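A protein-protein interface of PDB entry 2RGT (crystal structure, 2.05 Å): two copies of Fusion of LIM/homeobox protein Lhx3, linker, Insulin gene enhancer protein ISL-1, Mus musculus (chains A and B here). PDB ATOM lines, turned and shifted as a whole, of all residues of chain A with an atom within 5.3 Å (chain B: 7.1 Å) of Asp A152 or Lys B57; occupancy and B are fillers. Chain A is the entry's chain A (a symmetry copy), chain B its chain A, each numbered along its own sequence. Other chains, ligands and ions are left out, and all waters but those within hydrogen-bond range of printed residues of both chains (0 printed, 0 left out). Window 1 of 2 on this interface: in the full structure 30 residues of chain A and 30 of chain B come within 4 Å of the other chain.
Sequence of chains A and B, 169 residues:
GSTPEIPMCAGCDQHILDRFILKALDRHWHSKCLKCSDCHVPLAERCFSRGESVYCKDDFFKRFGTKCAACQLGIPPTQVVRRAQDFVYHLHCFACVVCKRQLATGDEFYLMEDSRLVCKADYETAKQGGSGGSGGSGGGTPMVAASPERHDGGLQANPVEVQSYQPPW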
ATOM      1  N   ARG A  83      33.830  -6.425  -0.199  1.00  0.00           N
ATOM      2  CA  ARG A  83      34.945  -6.202   0.703  1.00  0.00           C
ATOM      3  C   ARG A  83      35.475  -7.477   1.338  1.00  0.00           C
ATOM      4  O   ARG A  83      34.760  -8.470   1.426  1.00  0.00           O
ATOM      5  CB  ARG A  83      34.568  -5.153   1.739  1.00  0.00           C
ATOM      6  CG  ARG A  83      33.619  -5.592   2.751  1.00  0.00           C
ATOM      7  CD  ARG A  83      33.905  -4.804   4.027  1.00  0.00           C
ATOM      8  NE  ARG A  83      33.456  -3.398   4.035  1.00  0.00           N
ATOM      9  CZ  ARG A  83      34.141  -2.421   4.636  1.00  0.00           C
ATOM     10  NH1 ARG A  83      35.306  -2.677   5.243  1.00  0.00           N
ATOM     11  NH2 ARG A  83      33.688  -1.184   4.632  1.00  0.00           N
ATOM     12  N   GLU A 149      27.887  -4.432  -1.103  1.00  0.00           N
ATOM     13  CA  GLU A 149      27.253  -3.339  -0.398  1.00  0.00           C
ATOM     14  C   GLU A 149      27.667  -1.994  -0.928  1.00  0.00           C
ATOM     15  O   GLU A 149      28.793  -1.788  -1.388  1.00  0.00           O
ATOM     16  CB  GLU A 149      27.600  -3.399   1.091  1.00  0.00           C
ATOM     17  CG  GLU A 149      29.082  -3.632   1.328  1.00  0.00           C
ATOM     18  CD  GLU A 149      29.558  -3.074   2.648  1.00  0.00           C
ATOM     19  OE1 GLU A 149      28.714  -3.065   3.592  1.00  0.00           O
ATOM     20  OE2 GLU A 149      30.759  -2.631   2.726  1.00  0.00           O
ATOM     21  N   ARG A 150      26.741  -1.059  -0.801  1.00  0.00           N
ATOM     22  CA  ARG A 150      27.050   0.373  -0.859  1.00  0.00           C
ATOM     23  C   ARG A 150      28.253   0.743  -0.024  1.00  0.00           C
ATOM     24  O   ARG A 150      28.348   0.427   1.154  1.00  0.00           O
ATOM     25  CB  ARG A 150      25.858   1.168  -0.369  1.00  0.00           C
ATOM     26  CG  ARG A 150      24.575   0.694  -1.002  1.00  0.00           C
ATOM     27  CD  ARG A 150      24.421   1.366  -2.298  1.00  0.00           C
ATOM     28  NE  ARG A 150      23.067   1.149  -2.723  1.00  0.00           N
ATOM     29  CZ  ARG A 150      22.491   1.757  -3.744  1.00  0.00           C
ATOM     30  NH1 ARG A 150      23.182   2.664  -4.450  1.00  0.00           N
ATOM     31  NH2 ARG A 150      21.218   1.451  -4.033  1.00  0.00           N
ATOM     32  N   HIS A 151      29.195   1.433  -0.657  1.00  0.00           N
ATOM     33  CA  HIS A 151      30.499   1.682  -0.054  1.00  0.00           C
ATOM     34  C   HIS A 151      30.445   2.868   0.902  1.00  0.00           C
ATOM     35  O   HIS A 151      29.916   3.926   0.564  1.00  0.00           O
ATOM     36  CB  HIS A 151      31.552   1.926  -1.136  1.00  0.00           C
ATOM     37  CG  HIS A 151      32.736   2.710  -0.661  1.00  0.00           C
ATOM     38  ND1 HIS A 151      33.565   2.268   0.348  1.00  0.00           N
ATOM     39  CD2 HIS A 151      33.229   3.907  -1.056  1.00  0.00           C
ATOM     40  CE1 HIS A 151      34.518   3.159   0.554  1.00  0.00           C
ATOM     41  NE2 HIS A 151      34.338   4.164  -0.285  1.00  0.00           N
ATOM     42  N   ASP A 152      30.996   2.683   2.097  1.00  0.00           N
ATOM     43  CA  ASP A 152      30.632   3.505   3.244  1.00  0.00           C
ATOM     44  C   ASP A 152      31.637   4.632   3.457  1.00  0.00           C
ATOM     45  O   ASP A 152      31.758   5.170   4.557  1.00  0.00           O
ATOM     46  CB  ASP A 152      30.529   2.648   4.507  1.00  0.00           C
ATOM     47  CG  ASP A 152      31.832   1.952   4.846  1.00  0.00           C
ATOM     48  OD1 ASP A 152      32.893   2.609   4.784  1.00  0.00           O
ATOM     49  OD2 ASP A 152      31.796   0.747   5.176  1.00  0.00           O
ATOM     50  N   GLY A 153      32.278   4.993   2.388  1.00  0.00           N
ATOM     51  CA  GLY A 153      33.116   6.168   2.240  1.00  0.00           C
ATOM     52  C   GLY A 153      34.021   6.390   3.436  1.00  0.00           C
ATOM     53  O   GLY A 153      34.481   7.505   3.681  1.00  0.00           O
ATOM     54  N   GLY A 154      34.276   5.321   4.184  1.00  0.00           N
ATOM     55  CA  GLY A 154      35.418   5.272   5.078  1.00  0.00           C
ATOM     56  C   GLY A 154      35.000   5.356   6.531  1.00  0.00           C
ATOM     57  O   GLY A 154      35.547   6.140   7.306  1.00  0.00           O
ATOM     58  N   LEU A 155      34.022   4.536   6.897  1.00  0.00           N
ATOM     59  CA  LEU A 155      33.236   4.754   8.107  1.00  0.00           C
ATOM     60  C   LEU A 155      33.862   3.806   9.123  1.00  0.00           C
ATOM     61  O   LEU A 155      34.247   2.685   8.786  1.00  0.00           O
ATOM     62  CB  LEU A 155      31.742   4.636   7.803  1.00  0.00           C
ATOM     63  CG  LEU A 155      30.792   5.291   8.809  1.00  0.00           C
ATOM     64  CD1 LEU A 155      31.199   6.732   9.073  1.00  0.00           C
ATOM     65  CD2 LEU A 155      29.355   5.216   8.318  1.00  0.00           C
ATOM     66  N   CYS B  36      21.205  -5.565  16.201  1.00  0.00           N
ATOM     67  CA  CYS B  36      20.993  -4.135  16.152  1.00  0.00           C
ATOM     68  C   CYS B  36      20.167  -3.661  17.353  1.00  0.00           C
ATOM     69  O   CYS B  36      19.100  -4.194  17.645  1.00  0.00           O
ATOM     70  CB  CYS B  36      20.317  -3.732  14.842  1.00  0.00           C
ATOM     71  SG  CYS B  36      20.085  -1.933  14.671  1.00  0.00           S
ATOM     72  N   LEU B  43      23.940  -9.085  13.908  1.00  0.00           N
ATOM     73  CA  LEU B  43      25.061  -8.407  13.247  1.00  0.00           C
ATOM     74  C   LEU B  43      26.153  -9.396  12.856  1.00  0.00           C
ATOM     75  O   LEU B  43      26.563 -10.222  13.692  1.00  0.00           O
ATOM     76  CB  LEU B  43      25.602  -7.304  14.163  1.00  0.00           C
ATOM     77  CG  LEU B  43      24.523  -6.246  14.421  1.00  0.00           C
ATOM     78  CD1 LEU B  43      24.943  -5.208  15.445  1.00  0.00           C
ATOM     79  CD2 LEU B  43      24.177  -5.591  13.143  1.00  0.00           C
ATOM     80  N   ARG B  46      30.866  -6.952  10.356  1.00  0.00           N
ATOM     81  CA  ARG B  46      31.140  -5.660  11.005  1.00  0.00           C
ATOM     82  C   ARG B  46      29.881  -5.122  11.642  1.00  0.00           C
ATOM     83  O   ARG B  46      28.765  -5.512  11.283  1.00  0.00           O
ATOM     84  CB  ARG B  46      31.646  -4.612  10.006  1.00  0.00           C
ATOM     85  CG  ARG B  46      33.161  -4.369   9.995  1.00  0.00           C
ATOM     86  CD  ARG B  46      33.613  -3.834   8.636  1.00  0.00           C
ATOM     87  NE  ARG B  46      33.516  -4.919   7.661  1.00  0.00           N
ATOM     88  CZ  ARG B  46      32.482  -5.122   6.844  1.00  0.00           C
ATOM     89  NH1 ARG B  46      31.443  -4.278   6.835  1.00  0.00           N
ATOM     90  NH2 ARG B  46      32.510  -6.173   6.023  1.00  0.00           N
ATOM     91  N   CYS B  47      30.076  -4.209  12.582  1.00  0.00           N
ATOM     92  CA  CYS B  47      28.989  -3.440  13.145  1.00  0.00           C
ATOM     93  C   CYS B  47      29.463  -2.058  13.596  1.00  0.00           C
ATOM     94  O   CYS B  47      30.650  -1.816  13.806  1.00  0.00           O
ATOM     95  CB  CYS B  47      28.322  -4.202  14.301  1.00  0.00           C
ATOM     96  SG  CYS B  47      29.417  -4.442  15.632  1.00  0.00           S
ATOM     97  N   PHE B  48      28.495  -1.180  13.799  1.00  0.00           N
ATOM     98  CA  PHE B  48      28.756   0.211  14.096  1.00  0.00           C
ATOM     99  C   PHE B  48      28.241   0.522  15.478  1.00  0.00           C
ATOM    100  O   PHE B  48      27.248  -0.033  15.906  1.00  0.00           O
ATOM    101  CB  PHE B  48      28.082   1.082  13.044  1.00  0.00           C
ATOM    102  CG  PHE B  48      28.358   0.626  11.652  1.00  0.00           C
ATOM    103  CD1 PHE B  48      29.287   1.270  10.875  1.00  0.00           C
ATOM    104  CD2 PHE B  48      27.734  -0.488  11.146  1.00  0.00           C
ATOM    105  CE1 PHE B  48      29.557   0.835   9.611  1.00  0.00           C
ATOM    106  CE2 PHE B  48      28.006  -0.923   9.880  1.00  0.00           C
ATOM    107  CZ  PHE B  48      28.918  -0.262   9.116  1.00  0.00           C
ATOM    108  N   TYR B  55      24.707  -1.074  16.275  1.00  0.00           N
ATOM    109  CA  TYR B  55      23.707  -0.813  15.239  1.00  0.00           C
ATOM    110  C   TYR B  55      24.130  -1.500  13.955  1.00  0.00           C
ATOM    111  O   TYR B  55      25.325  -1.630  13.667  1.00  0.00           O
ATOM    112  CB  TYR B  55      23.559   0.691  14.986  1.00  0.00           C
ATOM    113  CG  TYR B  55      23.215   1.475  16.245  1.00  0.00           C
ATOM    114  CD1 TYR B  55      21.893   1.589  16.685  1.00  0.00           C
ATOM    115  CD2 TYR B  55      24.234   2.058  17.037  1.00  0.00           C
ATOM    116  CE1 TYR B  55      21.582   2.299  17.896  1.00  0.00           C
ATOM    117  CE2 TYR B  55      23.940   2.761  18.221  1.00  0.00           C
ATOM    118  CZ  TYR B  55      22.620   2.883  18.640  1.00  0.00           C
ATOM    119  OH  TYR B  55      22.347   3.586  19.797  1.00  0.00           O
ATOM    120  N   CYS B  56      23.145  -2.012  13.242  1.00  0.00           N
ATOM    121  CA  CYS B  56      23.276  -2.242  11.818  1.00  0.00           C
ATOM    122  C   CYS B  56      23.431  -0.899  11.078  1.00  0.00           C
ATOM    123  O   CYS B  56      22.999   0.138  11.562  1.00  0.00           O
ATOM    124  CB  CYS B  56      22.037  -2.959  11.306  1.00  0.00           C
ATOM    125  SG  CYS B  56      20.668  -1.816  10.868  1.00  0.00           S
ATOM    126  N   LYS B  57      24.020  -0.937   9.892  1.00  0.00           N
ATOM    127  CA  LYS B  57      24.268   0.255   9.068  1.00  0.00           C
ATOM    128  C   LYS B  57      23.068   1.191   8.808  1.00  0.00           C
ATOM    129  O   LYS B  57      23.190   2.391   8.964  1.00  0.00           O
ATOM    130  CB  LYS B  57      24.890  -0.208   7.732  1.00  0.00           C
ATOM    131  CG  LYS B  57      25.616   0.853   6.929  1.00  0.00           C
ATOM    132  CD  LYS B  57      26.162   0.236   5.618  1.00  0.00           C
ATOM    133  CE  LYS B  57      27.335   1.056   5.087  1.00  0.00           C
ATOM    134  NZ  LYS B  57      28.369   0.266   4.360  1.00  0.00           N
ATOM    135  N   ASP B  58      21.948   0.666   8.320  1.00  0.00           N
ATOM    136  CA  ASP B  58      20.737   1.467   8.114  1.00  0.00           C
ATOM    137  C   ASP B  58      20.489   2.324   9.369  1.00  0.00           C
ATOM    138  O   ASP B  58      20.508   3.564   9.326  1.00  0.00           O
ATOM    139  CB  ASP B  58      19.487   0.584   7.822  1.00  0.00           C
ATOM    140  CG  ASP B  58      19.545  -0.156   6.443  1.00  0.00           C
ATOM    141  OD1 ASP B  58      20.226   0.327   5.505  1.00  0.00           O
ATOM    142  OD2 ASP B  58      18.903  -1.241   6.287  1.00  0.00           O
ATOM    143  N   ASP B  59      20.268   1.645  10.495  1.00  0.00           N
ATOM    144  CA  ASP B  59      19.822   2.309  11.703  1.00  0.00           C
ATOM    145  C   ASP B  59      20.855   3.272  12.266  1.00  0.00           C
ATOM    146  O   ASP B  59      20.484   4.265  12.903  1.00  0.00           O
ATOM    147  CB  ASP B  59      19.378   1.305  12.766  1.00  0.00           C
ATOM    148  CG  ASP B  59      17.982   0.733  12.482  1.00  0.00           C
ATOM    149  OD1 ASP B  59      17.825  -0.513  12.539  1.00  0.00           O
ATOM    150  OD2 ASP B  59      17.033   1.514  12.230  1.00  0.00           O
ATOM    151  N   PHE B  60      22.134   2.997  12.012  1.00  0.00           N
ATOM    152  CA  PHE B  60      23.216   3.902  12.455  1.00  0.00           C
ATOM    153  C   PHE B  60      23.099   5.248  11.737  1.00  0.00           C
ATOM    154  O   PHE B  60      23.353   6.280  12.334  1.00  0.00           O
ATOM    155  CB  PHE B  60      24.602   3.287  12.216  1.00  0.00           C
ATOM    156  CG  PHE B  60      25.748   4.156  12.683  1.00  0.00           C
ATOM    157  CD1 PHE B  60      26.172   4.117  14.012  1.00  0.00           C
ATOM    158  CD2 PHE B  60      26.400   5.014  11.789  1.00  0.00           C
ATOM    159  CE1 PHE B  60      27.201   4.928  14.466  1.00  0.00           C
ATOM    160  CE2 PHE B  60      27.436   5.821  12.211  1.00  0.00           C
ATOM    161  CZ  PHE B  60      27.855   5.778  13.571  1.00  0.00           C
ATOM    162  N   PHE B  61      22.714   5.216  10.465  1.00  0.00           N
ATOM    163  CA  PHE B  61      22.677   6.421   9.645  1.00  0.00           C
ATOM    164  C   PHE B  61      21.379   7.192   9.859  1.00  0.00           C
ATOM    165  O   PHE B  61      21.342   8.415   9.720  1.00  0.00           O
ATOM    166  CB  PHE B  61      22.841   6.067   8.166  1.00  0.00           C
ATOM    167  CG  PHE B  61      24.272   5.933   7.730  1.00  0.00           C
ATOM    168  CD1 PHE B  61      25.222   6.856   8.132  1.00  0.00           C
ATOM    169  CD2 PHE B  61      24.667   4.883   6.917  1.00  0.00           C
ATOM    170  CE1 PHE B  61      26.540   6.735   7.733  1.00  0.00           C
ATOM    171  CE2 PHE B  61      25.983   4.758   6.515  1.00  0.00           C
ATOM    172  CZ  PHE B  61      26.920   5.685   6.924  1.00  0.00           C
ATOM    173  N   LYS B  62      20.316   6.447  10.144  1.00  0.00           N
ATOM    174  CA  LYS B  62      19.018   6.985  10.514  1.00  0.00           C
ATOM    175  C   LYS B  62      19.118   7.717  11.837  1.00  0.00           C
ATOM    176  O   LYS B  62      18.459   8.716  12.056  1.00  0.00           O
ATOM    177  CB  LYS B  62      18.011   5.848  10.670  1.00  0.00           C
ATOM    178  CG  LYS B  62      17.287   5.459   9.412  1.00  0.00           C
ATOM    179  CD  LYS B  62      17.100   3.964   9.324  1.00  0.00           C
ATOM    180  CE  LYS B  62      15.680   3.561   9.631  1.00  0.00           C
ATOM    181  NZ  LYS B  62      15.065   2.772   8.544  1.00  0.00           N
ATOM    182  N   ARG B  63      19.955   7.195  12.714  1.00  0.00           N
ATOM    183  CA  ARG B  63      20.067   7.700  14.078  1.00  0.00           C
ATOM    184  C   ARG B  63      21.107   8.811  14.171  1.00  0.00           C
ATOM    185  O   ARG B  63      20.840   9.880  14.719  1.00  0.00           O
ATOM    186  CB  ARG B  63      20.421   6.565  15.041  1.00  0.00           C
ATOM    187  CG  ARG B  63      20.332   6.948  16.510  1.00  0.00           C
ATOM    188  CD  ARG B  63      20.351   5.717  17.402  1.00  0.00           C
ATOM    189  NE  ARG B  63      19.013   5.170  17.607  1.00  0.00           N
ATOM    190  CZ  ARG B  63      18.125   5.667  18.462  1.00  0.00           C
ATOM    191  NH1 ARG B  63      18.431   6.726  19.197  1.00  0.00           N
ATOM    192  NH2 ARG B  63      16.931   5.103  18.582  1.00  0.00           N
ATOM    193  N   PRO B  76      20.288   8.718   4.928  1.00  0.00           N
ATOM    194  CA  PRO B  76      21.492   7.918   4.659  1.00  0.00           C
ATOM    195  C   PRO B  76      22.253   8.452   3.429  1.00  0.00           C
ATOM    196  O   PRO B  76      21.635   9.057   2.547  1.00  0.00           O
ATOM    197  CB  PRO B  76      20.890   6.539   4.336  1.00  0.00           C
ATOM    198  CG  PRO B  76      19.647   6.905   3.578  1.00  0.00           C
ATOM    199  CD  PRO B  76      19.070   8.019   4.441  1.00  0.00           C
ATOM    200  N   PRO B  77      23.562   8.138   3.314  1.00  0.00           N
ATOM    201  CA  PRO B  77      24.393   8.656   2.213  1.00  0.00           C
ATOM    202  C   PRO B  77      23.757   8.307   0.869  1.00  0.00           C
ATOM    203  O   PRO B  77      23.988   9.028  -0.098  1.00  0.00           O
ATOM    204  CB  PRO B  77      25.718   7.906   2.391  1.00  0.00           C
ATOM    205  CG  PRO B  77      25.739   7.573   3.817  1.00  0.00           C
ATOM    206  CD  PRO B  77      24.321   7.184   4.132  1.00  0.00           C
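No position is printed for both chains. Of the 5 pairs that touch across the chains among the printed residues, none has its exchanged pair printed and touching as well.
OE1 of Glu A149 lies within salt-bridge range of NZ of Lys B57 (3.4 Å). The side-chain amino group (NZ) of Lys B57 is in hydrogen-bond range of the backbone carbonyl oxygen (O) of Arg A150, 3.2 Å away. The side-chain amino group of Lys B57 lies within salt-bridge range of the side-chain carboxylate of Asp A152 (3.6 Å).
Among the printed residues, merely in contact across the chains: Arg A83 with Arg B46 and Leu A155 with Phe B61.
Of the 8 printed residues of chain A, 5 touch a printed residue of chain B. Hydrophobic or aromatic side chains of chain A that line the printed part of chain B: Leu A155. Hydrophobic or aromatic side chains of chain B within 4 Å of the printed part of chain A: Phe B61. Among the printed residues, Asp or Glu carboxylates within 4 Å of a Lys or Arg side-chain nitrogen of the other chain: Glu A149 with Lys B57 and Asp A152 with Lys B57.
Of the printed residues of chain B, Arg A83 touches Arg B46. Printed residues of chain B within 4 Å of Glu A149: Lys B57. Of chain B, only Lys B57 comes within 4 Å of Asp A152. Of the printed residues of chain A, Arg B46 touches Arg A83 (2.8 Å). Printed residues of chain A within 4 Å of Phe B61: Leu A155. The nearest residue of chain A that does not touch Lys B57 is His A151 (4.8 Å).
The side-chain carboxylate (OD1) of Asp A152 sits close to the backbone NH (N) of Gly A154 (3.1 Å). The side-chain carboxylate of Glu A149 lies within salt-bridge range of the guanidinium group of Arg A83 (3.1 Å). The side-chain carboxylate (OD1) of Asp A152 sits at hydrogen-bond distance from the backbone NH (N) of Leu A155. NH2 of Arg A83 is in salt-bridge range of OD2 of Asp A152.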
